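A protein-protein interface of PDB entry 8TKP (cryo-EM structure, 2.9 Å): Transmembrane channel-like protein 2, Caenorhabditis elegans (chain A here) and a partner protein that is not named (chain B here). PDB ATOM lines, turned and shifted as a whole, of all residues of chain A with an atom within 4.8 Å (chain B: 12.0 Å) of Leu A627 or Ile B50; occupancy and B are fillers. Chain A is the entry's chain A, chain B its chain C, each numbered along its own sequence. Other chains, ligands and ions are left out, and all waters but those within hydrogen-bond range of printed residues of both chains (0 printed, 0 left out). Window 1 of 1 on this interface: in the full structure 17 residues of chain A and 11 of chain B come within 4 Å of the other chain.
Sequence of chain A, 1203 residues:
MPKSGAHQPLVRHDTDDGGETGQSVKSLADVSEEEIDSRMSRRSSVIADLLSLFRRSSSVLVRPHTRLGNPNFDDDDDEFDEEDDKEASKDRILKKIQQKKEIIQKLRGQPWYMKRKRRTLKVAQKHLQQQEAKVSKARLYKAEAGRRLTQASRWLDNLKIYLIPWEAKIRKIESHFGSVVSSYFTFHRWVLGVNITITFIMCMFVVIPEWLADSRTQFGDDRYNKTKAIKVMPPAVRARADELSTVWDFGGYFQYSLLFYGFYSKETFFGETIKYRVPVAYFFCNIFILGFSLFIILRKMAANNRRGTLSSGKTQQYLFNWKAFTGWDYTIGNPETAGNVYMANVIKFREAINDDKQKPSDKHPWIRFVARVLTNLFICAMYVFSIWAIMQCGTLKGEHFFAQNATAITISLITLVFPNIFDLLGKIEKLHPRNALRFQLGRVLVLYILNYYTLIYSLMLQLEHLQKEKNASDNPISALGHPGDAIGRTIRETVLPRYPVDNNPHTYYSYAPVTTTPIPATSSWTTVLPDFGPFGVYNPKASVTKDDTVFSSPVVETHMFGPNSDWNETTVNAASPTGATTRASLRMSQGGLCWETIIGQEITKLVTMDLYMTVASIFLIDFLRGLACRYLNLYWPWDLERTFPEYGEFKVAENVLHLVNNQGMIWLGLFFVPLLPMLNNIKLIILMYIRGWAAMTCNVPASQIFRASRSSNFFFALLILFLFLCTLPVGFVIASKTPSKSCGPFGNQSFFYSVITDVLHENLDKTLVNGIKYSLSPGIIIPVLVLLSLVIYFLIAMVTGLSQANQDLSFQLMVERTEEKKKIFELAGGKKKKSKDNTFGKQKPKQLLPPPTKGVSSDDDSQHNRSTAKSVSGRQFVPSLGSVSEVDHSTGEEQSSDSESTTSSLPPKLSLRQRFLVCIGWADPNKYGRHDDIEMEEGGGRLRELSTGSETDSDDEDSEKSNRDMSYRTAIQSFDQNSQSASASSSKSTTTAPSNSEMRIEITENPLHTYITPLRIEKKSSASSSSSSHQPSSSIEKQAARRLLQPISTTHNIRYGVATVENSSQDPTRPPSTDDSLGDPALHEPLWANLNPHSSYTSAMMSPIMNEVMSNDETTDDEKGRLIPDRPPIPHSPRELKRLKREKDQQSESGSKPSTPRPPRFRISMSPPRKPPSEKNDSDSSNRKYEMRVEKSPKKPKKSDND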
ATOM      1  N   PHE A 623      19.899  13.195 -23.914  1.00  0.00           N
ATOM      2  CA  PHE A 623      18.895  12.180 -23.610  1.00  0.00           C
ATOM      3  C   PHE A 623      19.469  11.054 -22.755  1.00  0.00           C
ATOM      4  O   PHE A 623      18.955  10.760 -21.669  1.00  0.00           O
ATOM      5  CB  PHE A 623      18.308  11.628 -24.911  1.00  0.00           C
ATOM      6  CG  PHE A 623      17.330  10.510 -24.711  1.00  0.00           C
ATOM      7  CD1 PHE A 623      16.048  10.769 -24.260  1.00  0.00           C
ATOM      8  CD2 PHE A 623      17.687   9.202 -24.984  1.00  0.00           C
ATOM      9  CE1 PHE A 623      15.143   9.742 -24.077  1.00  0.00           C
ATOM     10  CE2 PHE A 623      16.786   8.172 -24.803  1.00  0.00           C
ATOM     11  CZ  PHE A 623      15.515   8.443 -24.348  1.00  0.00           C
ATOM     12  N   LEU A 624      20.528  10.402 -23.239  1.00  0.00           N
ATOM     13  CA  LEU A 624      21.099   9.278 -22.503  1.00  0.00           C
ATOM     14  C   LEU A 624      21.666   9.723 -21.163  1.00  0.00           C
ATOM     15  O   LEU A 624      21.536   9.011 -20.162  1.00  0.00           O
ATOM     16  CB  LEU A 624      22.170   8.583 -23.340  1.00  0.00           C
ATOM     17  CG  LEU A 624      21.633   7.629 -24.405  1.00  0.00           C
ATOM     18  CD1 LEU A 624      22.759   6.823 -25.026  1.00  0.00           C
ATOM     19  CD2 LEU A 624      20.581   6.707 -23.809  1.00  0.00           C
ATOM     20  N   ARG A 625      22.300  10.895 -21.122  1.00  0.00           N
ATOM     21  CA  ARG A 625      22.771  11.421 -19.845  1.00  0.00           C
ATOM     22  C   ARG A 625      21.606  11.698 -18.905  1.00  0.00           C
ATOM     23  O   ARG A 625      21.711  11.474 -17.695  1.00  0.00           O
ATOM     24  CB  ARG A 625      23.595  12.689 -20.055  1.00  0.00           C
ATOM     25  CG  ARG A 625      23.997  13.372 -18.760  1.00  0.00           C
ATOM     26  CD  ARG A 625      24.718  14.684 -19.003  1.00  0.00           C
ATOM     27  NE  ARG A 625      23.930  15.599 -19.819  1.00  0.00           N
ATOM     28  CZ  ARG A 625      24.197  16.890 -19.958  1.00  0.00           C
ATOM     29  NH1 ARG A 625      25.205  17.462 -19.320  1.00  0.00           N
ATOM     30  NH2 ARG A 625      23.432  17.627 -20.758  1.00  0.00           N
ATOM     31  N   GLY A 626      20.492  12.198 -19.440  1.00  0.00           N
ATOM     32  CA  GLY A 626      19.320  12.404 -18.607  1.00  0.00           C
ATOM     33  C   GLY A 626      18.806  11.110 -18.007  1.00  0.00           C
ATOM     34  O   GLY A 626      18.514  11.037 -16.810  1.00  0.00           O
ATOM     35  N   LEU A 627      18.701  10.066 -18.832  1.00  0.00           N
ATOM     36  CA  LEU A 627      18.266   8.769 -18.323  1.00  0.00           C
ATOM     37  C   LEU A 627      19.234   8.240 -17.273  1.00  0.00           C
ATOM     38  O   LEU A 627      18.813   7.698 -16.244  1.00  0.00           O
ATOM     39  CB  LEU A 627      18.129   7.768 -19.470  1.00  0.00           C
ATOM     40  CG  LEU A 627      16.951   7.954 -20.425  1.00  0.00           C
ATOM     41  CD1 LEU A 627      16.942   6.849 -21.467  1.00  0.00           C
ATOM     42  CD2 LEU A 627      15.642   7.978 -19.657  1.00  0.00           C
ATOM     43  N   ALA A 628      20.537   8.382 -17.522  1.00  0.00           N
ATOM     44  CA  ALA A 628      21.531   7.926 -16.559  1.00  0.00           C
ATOM     45  C   ALA A 628      21.372   8.651 -15.231  1.00  0.00           C
ATOM     46  O   ALA A 628      21.251   8.017 -14.178  1.00  0.00           O
ATOM     47  CB  ALA A 628      22.937   8.126 -17.122  1.00  0.00           C
ATOM     48  N   CYS A 629      21.332   9.984 -15.266  1.00  0.00           N
ATOM     49  CA  CYS A 629      21.207  10.754 -14.035  1.00  0.00           C
ATOM     50  C   CYS A 629      19.897  10.463 -13.318  1.00  0.00           C
ATOM     51  O   CYS A 629      19.830  10.559 -12.087  1.00  0.00           O
ATOM     52  CB  CYS A 629      21.325  12.247 -14.336  1.00  0.00           C
ATOM     53  SG  CYS A 629      22.920  12.739 -15.025  1.00  0.00           S
ATOM     54  N   ARG A 630      18.844  10.113 -14.058  1.00  0.00           N
ATOM     55  CA  ARG A 630      17.578   9.804 -13.407  1.00  0.00           C
ATOM     56  C   ARG A 630      17.596   8.434 -12.737  1.00  0.00           C
ATOM     57  O   ARG A 630      17.107   8.290 -11.610  1.00  0.00           O
ATOM     58  CB  ARG A 630      16.429   9.882 -14.410  1.00  0.00           C
ATOM     59  CG  ARG A 630      15.093   9.471 -13.819  1.00  0.00           C
ATOM     60  CD  ARG A 630      13.925   9.916 -14.673  1.00  0.00           C
ATOM     61  NE  ARG A 630      12.653   9.622 -14.027  1.00  0.00           N
ATOM     62  CZ  ARG A 630      11.478  10.069 -14.446  1.00  0.00           C
ATOM     63  NH1 ARG A 630      11.373  10.846 -15.512  1.00  0.00           N
ATOM     64  NH2 ARG A 630      10.379   9.734 -13.775  1.00  0.00           N
ATOM     65  N   TYR A 631      18.152   7.421 -13.398  1.00  0.00           N
ATOM     66  CA  TYR A 631      18.004   6.044 -12.937  1.00  0.00           C
ATOM     67  C   TYR A 631      19.225   5.502 -12.209  1.00  0.00           C
ATOM     68  O   TYR A 631      19.086   4.921 -11.128  1.00  0.00           O
ATOM     69  CB  TYR A 631      17.651   5.138 -14.125  1.00  0.00           C
ATOM     70  CG  TYR A 631      16.289   5.437 -14.706  1.00  0.00           C
ATOM     71  CD1 TYR A 631      15.135   4.975 -14.089  1.00  0.00           C
ATOM     72  CD2 TYR A 631      16.155   6.185 -15.867  1.00  0.00           C
ATOM     73  CE1 TYR A 631      13.888   5.249 -14.612  1.00  0.00           C
ATOM     74  CE2 TYR A 631      14.911   6.464 -16.399  1.00  0.00           C
ATOM     75  CZ  TYR A 631      13.781   5.993 -15.766  1.00  0.00           C
ATOM     76  OH  TYR A 631      12.539   6.266 -16.292  1.00  0.00           O
ATOM     77  N   LEU A 632      20.426   5.666 -12.767  1.00  0.00           N
ATOM     78  CA  LEU A 632      21.623   5.124 -12.138  1.00  0.00           C
ATOM     79  C   LEU A 632      22.047   5.905 -10.902  1.00  0.00           C
ATOM     80  O   LEU A 632      22.987   5.480 -10.220  1.00  0.00           O
ATOM     81  CB  LEU A 632      22.781   5.094 -13.140  1.00  0.00           C
ATOM     82  CG  LEU A 632      22.758   4.043 -14.253  1.00  0.00           C
ATOM     83  CD1 LEU A 632      22.394   2.673 -13.698  1.00  0.00           C
ATOM     84  CD2 LEU A 632      21.827   4.439 -15.390  1.00  0.00           C
ATOM     85  N   TYR A 647      21.241  17.470 -15.270  1.00  0.00           N
ATOM     86  CA  TYR A 647      20.432  16.930 -16.359  1.00  0.00           C
ATOM     87  C   TYR A 647      20.736  17.614 -17.686  1.00  0.00           C
ATOM     88  O   TYR A 647      20.558  17.004 -18.748  1.00  0.00           O
ATOM     89  CB  TYR A 647      18.945  17.054 -16.031  1.00  0.00           C
ATOM     90  CG  TYR A 647      18.425  15.969 -15.117  1.00  0.00           C
ATOM     91  CD1 TYR A 647      18.253  14.670 -15.579  1.00  0.00           C
ATOM     92  CD2 TYR A 647      18.098  16.242 -13.797  1.00  0.00           C
ATOM     93  CE1 TYR A 647      17.775  13.676 -14.749  1.00  0.00           C
ATOM     94  CE2 TYR A 647      17.618  15.255 -12.963  1.00  0.00           C
ATOM     95  CZ  TYR A 647      17.461  13.975 -13.441  1.00  0.00           C
ATOM     96  OH  TYR A 647      16.984  12.990 -12.606  1.00  0.00           O
ATOM     97  N   THR A 697      12.059  17.318 -23.336  1.00  0.00           N
ATOM     98  CA  THR A 697      12.154  16.023 -22.679  1.00  0.00           C
ATOM     99  C   THR A 697      13.455  15.811 -21.918  1.00  0.00           C
ATOM    100  O   THR A 697      13.484  14.981 -21.003  1.00  0.00           O
ATOM    101  CB  THR A 697      11.997  14.899 -23.710  1.00  0.00           C
ATOM    102  OG1 THR A 697      13.097  14.931 -24.625  1.00  0.00           O
ATOM    103  CG2 THR A 697      10.703  15.071 -24.485  1.00  0.00           C
ATOM    104  N   VAL B  42       6.102   7.490 -32.504  1.00  0.00           N
ATOM    105  CA  VAL B  42       5.772   7.193 -31.111  1.00  0.00           C
ATOM    106  C   VAL B  42       6.133   8.371 -30.212  1.00  0.00           C
ATOM    107  O   VAL B  42       5.342   8.788 -29.355  1.00  0.00           O
ATOM    108  CB  VAL B  42       6.472   5.900 -30.657  1.00  0.00           C
ATOM    109  CG1 VAL B  42       6.260   5.676 -29.173  1.00  0.00           C
ATOM    110  CG2 VAL B  42       5.950   4.714 -31.449  1.00  0.00           C
ATOM    111  N   CYS B  43       7.327   8.936 -30.401  1.00  0.00           N
ATOM    112  CA  CYS B  43       7.763  10.054 -29.573  1.00  0.00           C
ATOM    113  C   CYS B  43       6.946  11.314 -29.822  1.00  0.00           C
ATOM    114  O   CYS B  43       6.887  12.181 -28.945  1.00  0.00           O
ATOM    115  CB  CYS B  43       9.246  10.336 -29.807  1.00  0.00           C
ATOM    116  SG  CYS B  43      10.352   9.019 -29.253  1.00  0.00           S
ATOM    117  N   MET B  46       4.277  10.409 -27.160  1.00  0.00           N
ATOM    118  CA  MET B  46       4.596   9.985 -25.799  1.00  0.00           C
ATOM    119  C   MET B  46       4.545  11.148 -24.813  1.00  0.00           C
ATOM    120  O   MET B  46       3.978  11.015 -23.722  1.00  0.00           O
ATOM    121  CB  MET B  46       5.972   9.320 -25.762  1.00  0.00           C
ATOM    122  CG  MET B  46       6.005   7.936 -26.380  1.00  0.00           C
ATOM    123  SD  MET B  46       4.763   6.828 -25.683  1.00  0.00           S
ATOM    124  CE  MET B  46       5.272   6.781 -23.967  1.00  0.00           C
ATOM    125  N   ARG B  47       5.128  12.291 -25.177  1.00  0.00           N
ATOM    126  CA  ARG B  47       5.228  13.453 -24.289  1.00  0.00           C
ATOM    127  C   ARG B  47       5.907  13.078 -22.969  1.00  0.00           C
ATOM    128  O   ARG B  47       5.322  13.162 -21.887  1.00  0.00           O
ATOM    129  CB  ARG B  47       3.851  14.082 -24.045  1.00  0.00           C
ATOM    130  CG  ARG B  47       3.236  14.737 -25.267  1.00  0.00           C
ATOM    131  CD  ARG B  47       1.921  15.418 -24.918  1.00  0.00           C
ATOM    132  NE  ARG B  47       1.363  16.144 -26.054  1.00  0.00           N
ATOM    133  CZ  ARG B  47       0.231  16.834 -26.017  1.00  0.00           C
ATOM    134  NH1 ARG B  47      -0.495  16.914 -24.914  1.00  0.00           N
ATOM    135  NH2 ARG B  47      -0.181  17.462 -27.115  1.00  0.00           N
ATOM    136  N   ILE B  48       7.163  12.658 -23.080  1.00  0.00           N
ATOM    137  CA  ILE B  48       7.933  12.214 -21.928  1.00  0.00           C
ATOM    138  C   ILE B  48       8.652  13.403 -21.300  1.00  0.00           C
ATOM    139  O   ILE B  48       8.808  14.463 -21.910  1.00  0.00           O
ATOM    140  CB  ILE B  48       8.930  11.105 -22.317  1.00  0.00           C
ATOM    141  CG1 ILE B  48       9.809  11.567 -23.480  1.00  0.00           C
ATOM    142  CG2 ILE B  48       8.192   9.827 -22.678  1.00  0.00           C
ATOM    143  CD1 ILE B  48      10.783  10.518 -23.964  1.00  0.00           C
ATOM    144  N   ARG B  49       9.092  13.220 -20.057  1.00  0.00           N
ATOM    145  CA  ARG B  49       9.836  14.251 -19.336  1.00  0.00           C
ATOM    146  C   ARG B  49      10.810  13.551 -18.401  1.00  0.00           C
ATOM    147  O   ARG B  49      10.401  13.020 -17.363  1.00  0.00           O
ATOM    148  CB  ARG B  49       8.897  15.175 -18.566  1.00  0.00           C
ATOM    149  CG  ARG B  49       9.608  16.208 -17.710  1.00  0.00           C
ATOM    150  CD  ARG B  49      10.459  17.142 -18.553  1.00  0.00           C
ATOM    151  NE  ARG B  49      11.213  18.081 -17.729  1.00  0.00           N
ATOM    152  CZ  ARG B  49      12.020  19.018 -18.208  1.00  0.00           C
ATOM    153  NH1 ARG B  49      12.196  19.181 -19.508  1.00  0.00           N
ATOM    154  NH2 ARG B  49      12.670  19.809 -17.359  1.00  0.00           N
ATOM    155  N   ILE B  50      12.088  13.553 -18.763  1.00  0.00           N
ATOM    156  CA  ILE B  50      13.118  12.819 -18.027  1.00  0.00           C
ATOM    157  C   ILE B  50      13.503  13.533 -16.731  1.00  0.00           C
ATOM    158  O   ILE B  50      13.413  12.918 -15.659  1.00  0.00           O
ATOM    159  CB  ILE B  50      14.354  12.562 -18.906  1.00  0.00           C
ATOM    160  CG1 ILE B  50      14.116  11.385 -19.857  1.00  0.00           C
ATOM    161  CG2 ILE B  50      15.575  12.292 -18.045  1.00  0.00           C
ATOM    162  CD1 ILE B  50      13.284  11.716 -21.077  1.00  0.00           C
ATOM    163  N   PRO B  51      13.940  14.800 -16.754  1.00  0.00           N
ATOM    164  CA  PRO B  51      14.495  15.395 -15.532  1.00  0.00           C
ATOM    165  C   PRO B  51      13.468  15.498 -14.416  1.00  0.00           C
ATOM    166  O   PRO B  51      12.271  15.673 -14.649  1.00  0.00           O
ATOM    167  CB  PRO B  51      14.956  16.786 -15.987  1.00  0.00           C
ATOM    168  CG  PRO B  51      15.043  16.703 -17.464  1.00  0.00           C
ATOM    169  CD  PRO B  51      13.953  15.771 -17.861  1.00  0.00           C
ATOM    170  N   ARG B  52      13.959  15.384 -13.185  1.00  0.00           N
ATOM    171  CA  ARG B  52      13.138  15.546 -11.996  1.00  0.00           C
ATOM    172  C   ARG B  52      13.131  17.003 -11.558  1.00  0.00           C
ATOM    173  O   ARG B  52      14.080  17.752 -11.806  1.00  0.00           O
ATOM    174  CB  ARG B  52      13.661  14.675 -10.853  1.00  0.00           C
ATOM    175  CG  ARG B  52      14.028  13.257 -11.246  1.00  0.00           C
ATOM    176  CD  ARG B  52      12.826  12.332 -11.216  1.00  0.00           C
ATOM    177  NE  ARG B  52      13.216  10.941 -11.412  1.00  0.00           N
ATOM    178  CZ  ARG B  52      13.648  10.142 -10.446  1.00  0.00           C
ATOM    179  NH1 ARG B  52      13.765  10.566  -9.198  1.00  0.00           N
ATOM    180  NH2 ARG B  52      13.973   8.886 -10.740  1.00  0.00           N
ATOM    181  N   THR B  53      12.048  17.404 -10.901  1.00  0.00           N
ATOM    182  CA  THR B  53      11.990  18.726 -10.298  1.00  0.00           C
ATOM    183  C   THR B  53      12.784  18.739  -9.000  1.00  0.00           C
ATOM    184  O   THR B  53      13.108  17.691  -8.434  1.00  0.00           O
ATOM    185  CB  THR B  53      10.542  19.137 -10.025  1.00  0.00           C
ATOM    186  OG1 THR B  53      10.033  18.392  -8.913  1.00  0.00           O
ATOM    187  CG2 THR B  53       9.676  18.866 -11.245  1.00  0.00           C
ATOM    188  N   LYS B  54      13.105  19.948  -8.529  1.00  0.00           N
ATOM    189  CA  LYS B  54      13.841  20.069  -7.275  1.00  0.00           C
ATOM    190  C   LYS B  54      13.040  19.499  -6.112  1.00  0.00           C
ATOM    191  O   LYS B  54      13.609  18.928  -5.174  1.00  0.00           O
ATOM    192  CB  LYS B  54      14.204  21.531  -7.012  1.00  0.00           C
ATOM    193  CG  LYS B  54      15.238  21.708  -5.917  1.00  0.00           C
ATOM    194  CD  LYS B  54      16.546  21.032  -6.298  1.00  0.00           C
ATOM    195  CE  LYS B  54      17.469  20.892  -5.098  1.00  0.00           C
ATOM    196  NZ  LYS B  54      16.899  19.979  -4.070  1.00  0.00           N
ATOM    197  N   ARG B  55      11.713  19.651  -6.153  1.00  0.00           N
ATOM    198  CA  ARG B  55      10.865  19.014  -5.152  1.00  0.00           C
ATOM    199  C   ARG B  55      10.943  17.497  -5.245  1.00  0.00           C
ATOM    200  O   ARG B  55      10.748  16.802  -4.240  1.00  0.00           O
ATOM    201  CB  ARG B  55       9.420  19.486  -5.310  1.00  0.00           C
ATOM    202  CG  ARG B  55       9.233  20.983  -5.139  1.00  0.00           C
ATOM    203  CD  ARG B  55       7.772  21.374  -5.277  1.00  0.00           C
ATOM    204  NE  ARG B  55       7.571  22.808  -5.109  1.00  0.00           N
ATOM    205  CZ  ARG B  55       6.392  23.411  -5.169  1.00  0.00           C
ATOM    206  NH1 ARG B  55       5.279  22.734  -5.391  1.00  0.00           N
ATOM    207  NH2 ARG B  55       6.330  24.730  -5.000  1.00  0.00           N
ATOM    208  N   GLN B  56      11.209  16.965  -6.437  1.00  0.00           N
ATOM    209  CA  GLN B  56      11.419  15.535  -6.608  1.00  0.00           C
ATOM    210  C   GLN B  56      12.860  15.116  -6.352  1.00  0.00           C
ATOM    211  O   GLN B  56      13.147  13.915  -6.349  1.00  0.00           O
ATOM    212  CB  GLN B  56      11.005  15.109  -8.018  1.00  0.00           C
ATOM    213  CG  GLN B  56       9.526  15.288  -8.311  1.00  0.00           C
ATOM    214  CD  GLN B  56       9.198  15.109  -9.780  1.00  0.00           C
ATOM    215  OE1 GLN B  56      10.092  14.994 -10.618  1.00  0.00           O
ATOM    216  NE2 GLN B  56       7.910  15.087 -10.101  1.00  0.00           N
ATOM    217  N   ILE B  57      13.763  16.068  -6.139  1.00  0.00           N
ATOM    218  CA  ILE B  57      15.173  15.776  -5.932  1.00  0.00           C
ATOM    219  C   ILE B  57      15.555  15.847  -4.460  1.00  0.00           C
ATOM    220  O   ILE B  57      16.273  14.981  -3.963  1.00  0.00           O
ATOM    221  CB  ILE B  57      16.041  16.729  -6.780  1.00  0.00           C
ATOM    222  CG1 ILE B  57      16.050  16.279  -8.241  1.00  0.00           C
ATOM    223  CG2 ILE B  57      17.451  16.820  -6.218  1.00  0.00           C
ATOM    224  CD1 ILE B  57      16.454  14.832  -8.428  1.00  0.00           C
ATOM    225  N   ILE B  60      15.616  12.800  -1.782  1.00  0.00           N
ATOM    226  CA  ILE B  60      16.530  11.665  -1.795  1.00  0.00           C
ATOM    227  C   ILE B  60      17.310  11.519  -0.496  1.00  0.00           C
ATOM    228  O   ILE B  60      17.992  10.507  -0.306  1.00  0.00           O
ATOM    229  CB  ILE B  60      17.505  11.766  -2.988  1.00  0.00           C
ATOM    230  CG1 ILE B  60      18.418  12.987  -2.843  1.00  0.00           C
ATOM    231  CG2 ILE B  60      16.738  11.804  -4.303  1.00  0.00           C
ATOM    232  CD1 ILE B  60      19.845  12.651  -2.455  1.00  0.00           C
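Among the printed residues, pairs that only touch across the chains: Gly A626 with Ile B50, Leu A627 with Ile B50, Tyr A647 with Pro B51, Tyr A647 with Arg B52, Thr A697 with Ile B48, Thr A697 with Arg B49 and Thr A697 with Pro B51.
Leu A627 touches just one residue of chain B: Ile B50.
Of chain A, only Gly A626 (3.4 Å), Leu A627 (3.7 Å), Arg A630 (2.9 Å) and Thr A697 (3.0 Å) come within 4 Å of Ile B50.
No residue of chain B comes within 4 Å of Phe A623.
Of the printed residues of chain B, Gly A626 touches Ile B50 (3.4 Å).
No residue of chain B comes within 4 Å of Ala A628.
No residue of chain B comes within 4 Å of Cys A629.
Arg A630 touches just these residues of chain B: Arg B49, Ile B50 and Arg B52.
No residue of chain B comes within 4 Å of Leu A632.
Of the printed residues of chain B, Tyr A647 touches Pro B51 (3.7 Å) and Arg B52 (3.3 Å).
Printed residues of chain A within 4 Å of Pro B51: Tyr A647 (3.7 Å) and Thr A697 (3.3 Å).
Of the printed residues of chain A, Arg B52 touches Arg A630 and Tyr A647.
Printed residues of chain B within 4 Å of Thr A697: Ile B48, Arg B49, Ile B50 and Pro B51.
Of the printed residues of chain A, Arg B49 touches Arg A630 (3.0 Å) and Thr A697 (3.996 Å).
Arg B47 touches none of the printed residues of chain A.
Ile B60 touches none of the printed residues of chain A.
The nearest residue of chain B that does not touch Leu A627 is Ile B48 (7.0 Å).
The nearest residue of chain A that does not touch Ile B50 is Phe A623 (4.04 Å).
The nearest printed residue of chain B that does not touch Thr A697 is Arg B47 (5.4 Å).
The backbone carbonyl oxygen (O) of Arg B49 sits at hydrogen-bond distance from the guanidinium group (NH1) of Arg A630.
The guanidinium group (NH1) of Arg A630 is in hydrogen-bond range of the backbone carbonyl oxygen (O) of Ile B50, at 2.9 Å.
O of Arg A630 sits at hydrogen-bond distance from NH2 of Arg B52 (3.3 Å).
The backbone NH (N) of Ile B50 lies within hydrogen-bond range of the backbone carbonyl oxygen (O) of Thr A697 (3.0 Å).
Printed residues of chain A that touch a printed residue of chain B: Gly A626, Leu A627, Arg A630, Tyr A647 and Thr A697.
Hydrophobic or aromatic side chains of chain A within 4 Å of the printed part of chain B: Leu A627 and Tyr A647.
Printed residues of chain B that touch a printed residue of chain A: Ile B48, Arg B49, Ile B50, Pro B51 and Arg B52.
Hydrophobic or aromatic side chains of chain B that line the printed part of chain A: Ile B48, Ile B50 and Pro B51.
Among the printed residues, no Asp or Glu carboxylate lies within 4 Å of a Lys or Arg side-chain nitrogen of the other chain.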
